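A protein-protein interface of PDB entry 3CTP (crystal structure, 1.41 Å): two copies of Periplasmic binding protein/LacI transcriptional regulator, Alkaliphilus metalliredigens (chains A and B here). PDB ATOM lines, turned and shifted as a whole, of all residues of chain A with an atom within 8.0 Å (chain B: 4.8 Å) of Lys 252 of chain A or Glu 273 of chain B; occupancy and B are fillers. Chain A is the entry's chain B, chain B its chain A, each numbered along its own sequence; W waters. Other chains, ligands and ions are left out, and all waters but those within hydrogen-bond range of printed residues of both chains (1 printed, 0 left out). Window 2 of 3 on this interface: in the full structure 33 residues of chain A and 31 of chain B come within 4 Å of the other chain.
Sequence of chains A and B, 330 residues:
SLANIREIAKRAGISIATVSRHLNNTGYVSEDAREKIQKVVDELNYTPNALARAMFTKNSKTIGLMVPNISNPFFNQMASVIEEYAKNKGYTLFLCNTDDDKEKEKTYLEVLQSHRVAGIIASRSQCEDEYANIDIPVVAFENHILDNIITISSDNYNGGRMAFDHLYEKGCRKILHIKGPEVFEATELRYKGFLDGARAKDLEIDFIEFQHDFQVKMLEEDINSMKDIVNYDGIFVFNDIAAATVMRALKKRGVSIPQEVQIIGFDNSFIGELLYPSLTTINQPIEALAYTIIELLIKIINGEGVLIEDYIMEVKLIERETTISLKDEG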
ATOM      1  N   VAL A 216      -4.985  -4.776   5.125  1.00  0.00           N
ATOM      2  CA  VAL A 216      -3.532  -4.782   5.229  1.00  0.00           C
ATOM      3  C   VAL A 216      -2.896  -4.103   4.013  1.00  0.00           C
ATOM      4  O   VAL A 216      -1.864  -3.429   4.112  1.00  0.00           O
ATOM      5  CB  VAL A 216      -3.025  -6.183   5.463  1.00  0.00           C
ATOM      6  CG1 VAL A 216      -1.511  -6.238   5.425  1.00  0.00           C
ATOM      7  CG2 VAL A 216      -3.554  -6.670   6.825  1.00  0.00           C
ATOM      8  N   MET A 218      -3.685  -1.438   2.688  1.00  0.00           N
ATOM      9  CA  MET A 218      -3.600   0.012   2.905  1.00  0.00           C
ATOM     10  C   MET A 218      -2.195   0.442   3.275  1.00  0.00           C
ATOM     11  O   MET A 218      -1.808   1.595   3.071  1.00  0.00           O
ATOM     12  CB  MET A 218      -4.536   0.459   4.037  1.00  0.00           C
ATOM     13  CG  MET A 218      -5.892   0.880   3.618  1.00  0.00           C
ATOM     14  SD  MET A 218      -6.777   1.750   4.951  1.00  0.00           S
ATOM     15  CE  MET A 218      -8.375   1.866   4.103  1.00  0.00           C
ATOM     16  N   LEU A 219      -1.419  -0.470   3.858  1.00  0.00           N
ATOM     17  CA  LEU A 219      -0.076  -0.102   4.285  1.00  0.00           C
ATOM     18  C   LEU A 219       0.863   0.155   3.099  1.00  0.00           C
ATOM     19  O   LEU A 219       1.946   0.752   3.275  1.00  0.00           O
ATOM     20  CB  LEU A 219       0.488  -1.195   5.209  1.00  0.00           C
ATOM     21  CG  LEU A 219      -0.368  -1.390   6.466  1.00  0.00           C
ATOM     22  CD1 LEU A 219       0.215  -2.476   7.359  1.00  0.00           C
ATOM     23  CD2 LEU A 219      -0.471  -0.101   7.276  1.00  0.00           C
ATOM     24  N   GLU A 220       0.454  -0.284   1.901  1.00  0.00           N
ATOM     25  CA  GLU A 220       1.235  -0.102   0.660  1.00  0.00           C
ATOM     26  C   GLU A 220       0.529   0.865  -0.300  1.00  0.00           C
ATOM     27  O   GLU A 220       0.882   0.928  -1.493  1.00  0.00           O
ATOM     28  CB  GLU A 220       1.460  -1.441  -0.052  1.00  0.00           C
ATOM     29  CG  GLU A 220       2.274  -2.449   0.758  1.00  0.00           C
ATOM     30  CD  GLU A 220       2.988  -3.484  -0.108  1.00  0.00           C
ATOM     31  OE1 GLU A 220       2.427  -3.906  -1.150  1.00  0.00           O
ATOM     32  OE2 GLU A 220       4.112  -3.886   0.263  1.00  0.00           O
ATOM     33  N   ASP A 222      -0.766   4.936  -1.087  1.00  0.00           N
ATOM     34  CA  ASP A 222      -0.479   6.348  -0.779  1.00  0.00           C
ATOM     35  C   ASP A 222      -1.739   7.180  -0.933  1.00  0.00           C
ATOM     36  O   ASP A 222      -2.631   6.803  -1.683  1.00  0.00           O
ATOM     37  CB  ASP A 222       0.499   6.925  -1.810  1.00  0.00           C
ATOM     38  CG  ASP A 222       1.918   7.049  -1.295  1.00  0.00           C
ATOM     39  OD1 ASP A 222       2.405   6.108  -0.639  1.00  0.00           O
ATOM     40  OD2 ASP A 222       2.556   8.094  -1.582  1.00  0.00           O
ATOM     41  N   MET A 226      -0.120  13.579  -0.453  1.00  0.00           N
ATOM     42  CA  MET A 226       0.123  13.346   0.963  1.00  0.00           C
ATOM     43  C   MET A 226       1.006  14.452   1.547  1.00  0.00           C
ATOM     44  O   MET A 226       0.817  14.895   2.681  1.00  0.00           O
ATOM     45  CB  MET A 226       0.809  11.991   1.164  1.00  0.00           C
ATOM     46  CG  MET A 226       1.035  11.638   2.608  1.00  0.00           C
ATOM     47  SD  MET A 226      -0.471  11.153   3.441  1.00  0.00           S
ATOM     48  CE  MET A 226      -0.167  11.883   5.064  1.00  0.00           C
ATOM     49  N   ALA A 244      -4.629   5.221  12.572  1.00  0.00           N
ATOM     50  CA  ALA A 244      -3.268   4.692  12.716  1.00  0.00           C
ATOM     51  C   ALA A 244      -2.528   4.713  11.392  1.00  0.00           C
ATOM     52  O   ALA A 244      -1.313   4.984  11.360  1.00  0.00           O
ATOM     53  CB  ALA A 244      -3.300   3.256  13.257  1.00  0.00           C
ATOM     54  N   THR A 245      -3.234   4.395  10.300  1.00  0.00           N
ATOM     55  CA  THR A 245      -2.573   4.382   8.990  1.00  0.00           C
ATOM     56  C   THR A 245      -2.203   5.790   8.553  1.00  0.00           C
ATOM     57  O   THR A 245      -1.137   6.009   7.966  1.00  0.00           O
ATOM     58  CB  THR A 245      -3.435   3.709   7.865  1.00  0.00           C
ATOM     59  OG1 THR A 245      -4.552   4.558   7.518  1.00  0.00           O
ATOM     60  CG2 THR A 245      -3.898   2.338   8.324  1.00  0.00           C
ATOM     61  N   VAL A 246      -3.084   6.739   8.850  1.00  0.00           N
ATOM     62  CA  VAL A 246      -2.817   8.134   8.508  1.00  0.00           C
ATOM     63  C   VAL A 246      -1.621   8.636   9.304  1.00  0.00           C
ATOM     64  O   VAL A 246      -0.734   9.299   8.771  1.00  0.00           O
ATOM     65  CB  VAL A 246      -4.062   9.002   8.776  1.00  0.00           C
ATOM     66  CG1 VAL A 246      -3.708  10.507   8.623  1.00  0.00           C
ATOM     67  CG2 VAL A 246      -5.174   8.618   7.844  1.00  0.00           C
ATOM     68  N   MET A 247      -1.568   8.306  10.588  1.00  0.00           N
ATOM     69  CA  MET A 247      -0.453   8.756  11.428  1.00  0.00           C
ATOM     70  C   MET A 247       0.857   8.125  10.962  1.00  0.00           C
ATOM     71  O   MET A 247       1.906   8.755  11.014  1.00  0.00           O
ATOM     72  CB  MET A 247      -0.726   8.380  12.894  1.00  0.00           C
ATOM     73  CG  MET A 247      -1.831   9.225  13.536  1.00  0.00           C
ATOM     74  SD  MET A 247      -2.178   8.924  15.312  1.00  0.00           S
ATOM     75  CE  MET A 247      -0.561   9.156  16.106  1.00  0.00           C
ATOM     76  N   ARG A 248       0.807   6.872  10.541  1.00  0.00           N
ATOM     77  CA  ARG A 248       2.031   6.232  10.001  1.00  0.00           C
ATOM     78  C   ARG A 248       2.537   6.995   8.786  1.00  0.00           C
ATOM     79  O   ARG A 248       3.729   7.254   8.649  1.00  0.00           O
ATOM     80  CB  ARG A 248       1.738   4.803   9.572  1.00  0.00           C
ATOM     81  CG  ARG A 248       2.805   4.200   8.616  1.00  0.00           C
ATOM     82  CD  ARG A 248       2.375   2.782   8.274  1.00  0.00           C
ATOM     83  NE  ARG A 248       3.286   2.068   7.383  1.00  0.00           N
ATOM     84  CZ  ARG A 248       3.114   1.974   6.072  1.00  0.00           C
ATOM     85  NH1 ARG A 248       2.072   2.560   5.495  1.00  0.00           N
ATOM     86  NH2 ARG A 248       3.979   1.273   5.336  1.00  0.00           N
ATOM     87  N   ALA A 249       1.627   7.358   7.894  1.00  0.00           N
ATOM     88  CA  ALA A 249       2.031   8.127   6.700  1.00  0.00           C
ATOM     89  C   ALA A 249       2.640   9.461   7.081  1.00  0.00           C
ATOM     90  O   ALA A 249       3.651   9.886   6.512  1.00  0.00           O
ATOM     91  CB  ALA A 249       0.856   8.329   5.770  1.00  0.00           C
ATOM     92  N   LEU A 250       2.018  10.151   8.027  1.00  0.00           N
ATOM     93  CA  LEU A 250       2.563  11.426   8.469  1.00  0.00           C
ATOM     94  C   LEU A 250       3.933  11.218   9.079  1.00  0.00           C
ATOM     95  O   LEU A 250       4.873  11.987   8.797  1.00  0.00           O
ATOM     96  CB  LEU A 250       1.621  12.087   9.481  1.00  0.00           C
ATOM     97  CG  LEU A 250       0.300  12.613   8.913  1.00  0.00           C
ATOM     98  CD1 LEU A 250      -0.682  12.984  10.027  1.00  0.00           C
ATOM     99  CD2 LEU A 250       0.561  13.828   8.010  1.00  0.00           C
ATOM    100  N   LYS A 251       4.077  10.199   9.926  1.00  0.00           N
ATOM    101  CA  LYS A 251       5.373   9.962  10.581  1.00  0.00           C
ATOM    102  C   LYS A 251       6.464   9.656   9.543  1.00  0.00           C
ATOM    103  O   LYS A 251       7.615  10.108   9.680  1.00  0.00           O
ATOM    104  CB  LYS A 251       5.264   8.827  11.599  1.00  0.00           C
ATOM    105  CG  LYS A 251       4.527   9.195  12.871  1.00  0.00           C
ATOM    106  CD  LYS A 251       4.161   7.923  13.642  1.00  0.00           C
ATOM    107  CE  LYS A 251       3.306   8.223  14.853  1.00  0.00           C
ATOM    108  NZ  LYS A 251       4.145   8.504  16.054  1.00  0.00           N
ATOM    109  N   LYS A 252       6.129   8.881   8.514  1.00  0.00           N
ATOM    110  CA  LYS A 252       7.130   8.561   7.485  1.00  0.00           C
ATOM    111  C   LYS A 252       7.680   9.841   6.850  1.00  0.00           C
ATOM    112  O   LYS A 252       8.796   9.862   6.313  1.00  0.00           O
ATOM    113  CB  LYS A 252       6.540   7.647   6.410  1.00  0.00           C
ATOM    114  CG  LYS A 252       6.521   6.177   6.807  1.00  0.00           C
ATOM    115  CD  LYS A 252       5.674   5.347   5.847  1.00  0.00           C
ATOM    116  CE  LYS A 252       6.308   3.990   5.610  1.00  0.00           C
ATOM    117  NZ  LYS A 252       6.900   3.440   6.861  1.00  0.00           N
ATOM    118  N   ARG A 253       6.901  10.908   6.916  1.00  0.00           N
ATOM    119  CA  ARG A 253       7.302  12.175   6.310  1.00  0.00           C
ATOM    120  C   ARG A 253       7.883  13.135   7.332  1.00  0.00           C
ATOM    121  O   ARG A 253       8.167  14.287   7.012  1.00  0.00           O
ATOM    122  CB  ARG A 253       6.123  12.838   5.610  1.00  0.00           C
ATOM    123  CG  ARG A 253       5.550  12.031   4.470  1.00  0.00           C
ATOM    124  CD  ARG A 253       4.623  12.876   3.623  1.00  0.00           C
ATOM    125  NE  ARG A 253       5.337  13.972   2.971  1.00  0.00           N
ATOM    126  CZ  ARG A 253       5.819  13.921   1.733  1.00  0.00           C
ATOM    127  NH1 ARG A 253       5.666  12.824   1.002  1.00  0.00           N
ATOM    128  NH2 ARG A 253       6.457  14.965   1.225  1.00  0.00           N
ATOM    129  N   GLY A 254       8.055  12.675   8.562  1.00  0.00           N
ATOM    130  CA  GLY A 254       8.681  13.516   9.589  1.00  0.00           C
ATOM    131  C   GLY A 254       7.761  14.521  10.262  1.00  0.00           C
ATOM    132  O   GLY A 254       8.230  15.459  10.917  1.00  0.00           O
ATOM    133  N   VAL A 255       6.448  14.334  10.119  1.00  0.00           N
ATOM    134  CA  VAL A 255       5.491  15.258  10.710  1.00  0.00           C
ATOM    135  C   VAL A 255       5.378  15.001  12.203  1.00  0.00           C
ATOM    136  O   VAL A 255       5.324  13.838  12.620  1.00  0.00           O
ATOM    137  CB  VAL A 255       4.097  15.126  10.054  1.00  0.00           C
ATOM    138  CG1 VAL A 255       3.069  15.907  10.829  1.00  0.00           C
ATOM    139  CG2 VAL A 255       4.146  15.623   8.612  1.00  0.00           C
ATOM    140  N   SER B 269       3.453  -9.824  11.090  1.00  0.00           N
ATOM    141  CA  SER B 269       2.048  -9.422  11.023  1.00  0.00           C
ATOM    142  C   SER B 269       1.923  -7.897  10.797  1.00  0.00           C
ATOM    143  O   SER B 269       2.913  -7.139  10.879  1.00  0.00           O
ATOM    144  CB  SER B 269       1.302  -9.836  12.292  1.00  0.00           C
ATOM    145  OG  SER B 269       1.752  -9.078  13.405  1.00  0.00           O
ATOM    146  N   PHE B 270       0.719  -7.434  10.478  1.00  0.00           N
ATOM    147  CA  PHE B 270       0.646  -6.065  10.001  1.00  0.00           C
ATOM    148  C   PHE B 270       1.024  -5.026  11.038  1.00  0.00           C
ATOM    149  O   PHE B 270       1.381  -3.899  10.693  1.00  0.00           O
ATOM    150  CB  PHE B 270      -0.733  -5.764   9.370  1.00  0.00           C
ATOM    151  CG  PHE B 270      -1.877  -5.662  10.354  1.00  0.00           C
ATOM    152  CD1 PHE B 270      -2.038  -4.515  11.123  1.00  0.00           C
ATOM    153  CD2 PHE B 270      -2.851  -6.669  10.423  1.00  0.00           C
ATOM    154  CE1 PHE B 270      -3.135  -4.373  12.025  1.00  0.00           C
ATOM    155  CE2 PHE B 270      -3.950  -6.546  11.304  1.00  0.00           C
ATOM    156  CZ  PHE B 270      -4.083  -5.390  12.111  1.00  0.00           C
ATOM    157  N   ILE B 271       0.975  -5.385  12.312  1.00  0.00           N
ATOM    158  CA  ILE B 271       1.260  -4.394  13.349  1.00  0.00           C
ATOM    159  C   ILE B 271       2.694  -3.885  13.267  1.00  0.00           C
ATOM    160  O   ILE B 271       2.985  -2.736  13.645  1.00  0.00           O
ATOM    161  CB  ILE B 271       0.940  -4.962  14.761  1.00  0.00           C
ATOM    162  CG1 ILE B 271       0.953  -3.849  15.809  1.00  0.00           C
ATOM    163  CG2 ILE B 271       1.902  -6.059  15.129  1.00  0.00           C
ATOM    164  CD1 ILE B 271      -0.246  -2.900  15.663  1.00  0.00           C
ATOM    165  N   GLY B 272       3.605  -4.714  12.780  1.00  0.00           N
ATOM    166  CA  GLY B 272       5.015  -4.299  12.685  1.00  0.00           C
ATOM    167  C   GLY B 272       5.289  -3.217  11.643  1.00  0.00           C
ATOM    168  O   GLY B 272       6.269  -2.454  11.755  1.00  0.00           O
ATOM    169  N   GLU B 273       4.417  -3.116  10.642  1.00  0.00           N
ATOM    170  CA  GLU B 273       4.579  -2.119   9.593  1.00  0.00           C
ATOM    171  C   GLU B 273       3.734  -0.901   9.910  1.00  0.00           C
ATOM    172  O   GLU B 273       4.034   0.242   9.537  1.00  0.00           O
ATOM    173  CB  GLU B 273       4.209  -2.736   8.231  1.00  0.00           C
ATOM    174  CG  GLU B 273       4.431  -1.807   7.034  1.00  0.00           C
ATOM    175  CD  GLU B 273       5.805  -1.130   7.016  1.00  0.00           C
ATOM    176  OE1 GLU B 273       6.831  -1.846   6.957  1.00  0.00           O
ATOM    177  OE2 GLU B 273       5.856   0.130   7.036  1.00  0.00           O
ATOM    178  N   LEU B 274       2.673  -1.133  10.655  1.00  0.00           N
ATOM    179  CA  LEU B 274       1.752  -0.080  10.952  1.00  0.00           C
ATOM    180  C   LEU B 274       2.387   0.900  11.919  1.00  0.00           C
ATOM    181  O   LEU B 274       2.191   2.115  11.775  1.00  0.00           O
ATOM    182  CB  LEU B 274       0.488  -0.694  11.556  1.00  0.00           C
ATOM    183  CG  LEU B 274      -0.598   0.293  11.903  1.00  0.00           C
ATOM    184  CD1 LEU B 274      -0.930   1.129  10.691  1.00  0.00           C
ATOM    185  CD2 LEU B 274      -1.790  -0.506  12.371  1.00  0.00           C
ATOM    186  N   LEU B 275       3.166   0.394  12.876  1.00  0.00           N
ATOM    187  CA  LEU B 275       3.863   1.238  13.873  1.00  0.00           C
ATOM    188  C   LEU B 275       5.315   1.692  13.530  1.00  0.00           C
ATOM    189  O   LEU B 275       5.883   1.270  12.539  1.00  0.00           O
ATOM    190  CB  LEU B 275       3.874   0.558  15.241  1.00  0.00           C
ATOM    191  CG  LEU B 275       4.616  -0.798  15.334  1.00  0.00           C
ATOM    192  CD1 LEU B 275       5.995  -0.798  14.675  1.00  0.00           C
ATOM    193  CD2 LEU B 275       4.762  -1.192  16.764  1.00  0.00           C
ATOM    194  N   SER B 278       9.356   1.050  12.153  1.00  0.00           N
ATOM    195  CA  SER B 278       8.840  -0.246  11.735  1.00  0.00           C
ATOM    196  C   SER B 278       9.722  -1.379  12.260  1.00  0.00           C
ATOM    197  O   SER B 278      10.926  -1.222  12.411  1.00  0.00           O
ATOM    198  CB  SER B 278       8.722  -0.323  10.227  1.00  0.00           C
ATOM    199  OG  SER B 278       9.998  -0.008   9.654  1.00  0.00           O
ATOM    200  N   ARG B 320      13.906  -4.175   9.261  1.00  0.00           N
ATOM    201  CA  ARG B 320      13.267  -2.878   9.191  1.00  0.00           C
ATOM    202  C   ARG B 320      14.018  -1.886  10.077  1.00  0.00           C
ATOM    203  O   ARG B 320      15.250  -1.892  10.082  1.00  0.00           O
ATOM    204  CB  ARG B 320      11.797  -2.973   9.562  1.00  0.00           C
ATOM    205  CG  ARG B 320      11.017  -3.939   8.674  1.00  0.00           C
ATOM    206  CD  ARG B 320       9.538  -3.682   8.826  1.00  0.00           C
ATOM    207  NE  ARG B 320       8.714  -4.493   7.932  1.00  0.00           N
ATOM    208  CZ  ARG B 320       7.878  -5.440   8.354  1.00  0.00           C
ATOM    209  NH1 ARG B 320       7.785  -5.742   9.657  1.00  0.00           N
ATOM    210  NH2 ARG B 320       7.131  -6.082   7.470  1.00  0.00           N
HETATM  211  O   HOH W   1       0.797   4.125  12.997  1.00  0.00           O
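The side-chain carboxylate of Glu 273 of chain B is in salt-bridge range of the guanidinium group of Arg 248 of chain A, 2.8 Å away. The side-chain amino group (NZ) of Lys 252 of chain A is in salt-bridge range of the side-chain carboxylate (OE2) of Glu 273 of chain B (3.5 Å).
The side-chain carboxylate (OE1) of Glu 273 of chain B is in salt-bridge range of the guanidinium group (NE) of Arg 320 of chain B (3.4 Å). O of Leu 219 of chain A lies within hydrogen-bond range of NH1 of Arg 248 of chain A (2.9 Å).
Among the printed residues, pairs that only touch across the chains: Val 216 of chain A with Phe 270 of chain B (3.7 Å), Leu 219 of chain A with Phe 270 of chain B (3.8 Å), Leu 219 of chain A with Leu 274 of chain B (3.7 Å), Ala 244 of chain A with Leu 274 of chain B (3.9 Å), Thr 245 of chain A with Leu 274 of chain B (3.98 Å) and Arg 248 of chain A with Leu 274 of chain B (3.5 Å).
Of chain B, only Glu 273 (3.5 Å) comes within 4 Å of Lys 252 of chain A. No residue of chain A comes within 4 Å of Gly 272 of chain B. Printed residues of chain B within 4 Å of Ala 244 of chain A: Leu 274 (3.9 Å). Printed residues of chain B within 4 Å of Arg 248 of chain A: Glu 273 and Leu 274. Printed residues of chain A within 4 Å of Phe 270 of chain B: Val 216 (3.7 Å) and Leu 219 (3.8 Å). Of the printed residues of chain B, Val 216 of chain A touches Phe 270 (3.7 Å). Of the printed residues of chain B, Leu 219 of chain A touches Phe 270 (3.8 Å) and Leu 274 (3.7 Å). The nearest printed residue of chain B that does not touch Lys 252 of chain A is Ser 278 of chain B (5.4 Å). The nearest residue of chain A that does not touch Glu 273 of chain B is Leu 219 of chain A (4.1 Å). The nearest printed residue of chain B that does not touch Val 216 of chain A is Ser 269 of chain B (6.6 Å).
Of the 18 printed residues of chain A, 6 touch a printed residue of chain B. Hydrophobic or aromatic side chains of chain A within 4 Å of the printed part of chain B: Val 216 and Leu 219. Among the printed residues, 8 pairs touch across the chains.
No position is printed for both chains. Of the 8 pairs that touch across the chains among the printed residues, none has its exchanged pair printed and touching as well.
Water W1 bridges the backbone carbonyl oxygen of Leu 274 of chain B (2.7 Å) and the backbone carbonyl oxygen of Ala 244 of chain A (2.8 Å).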
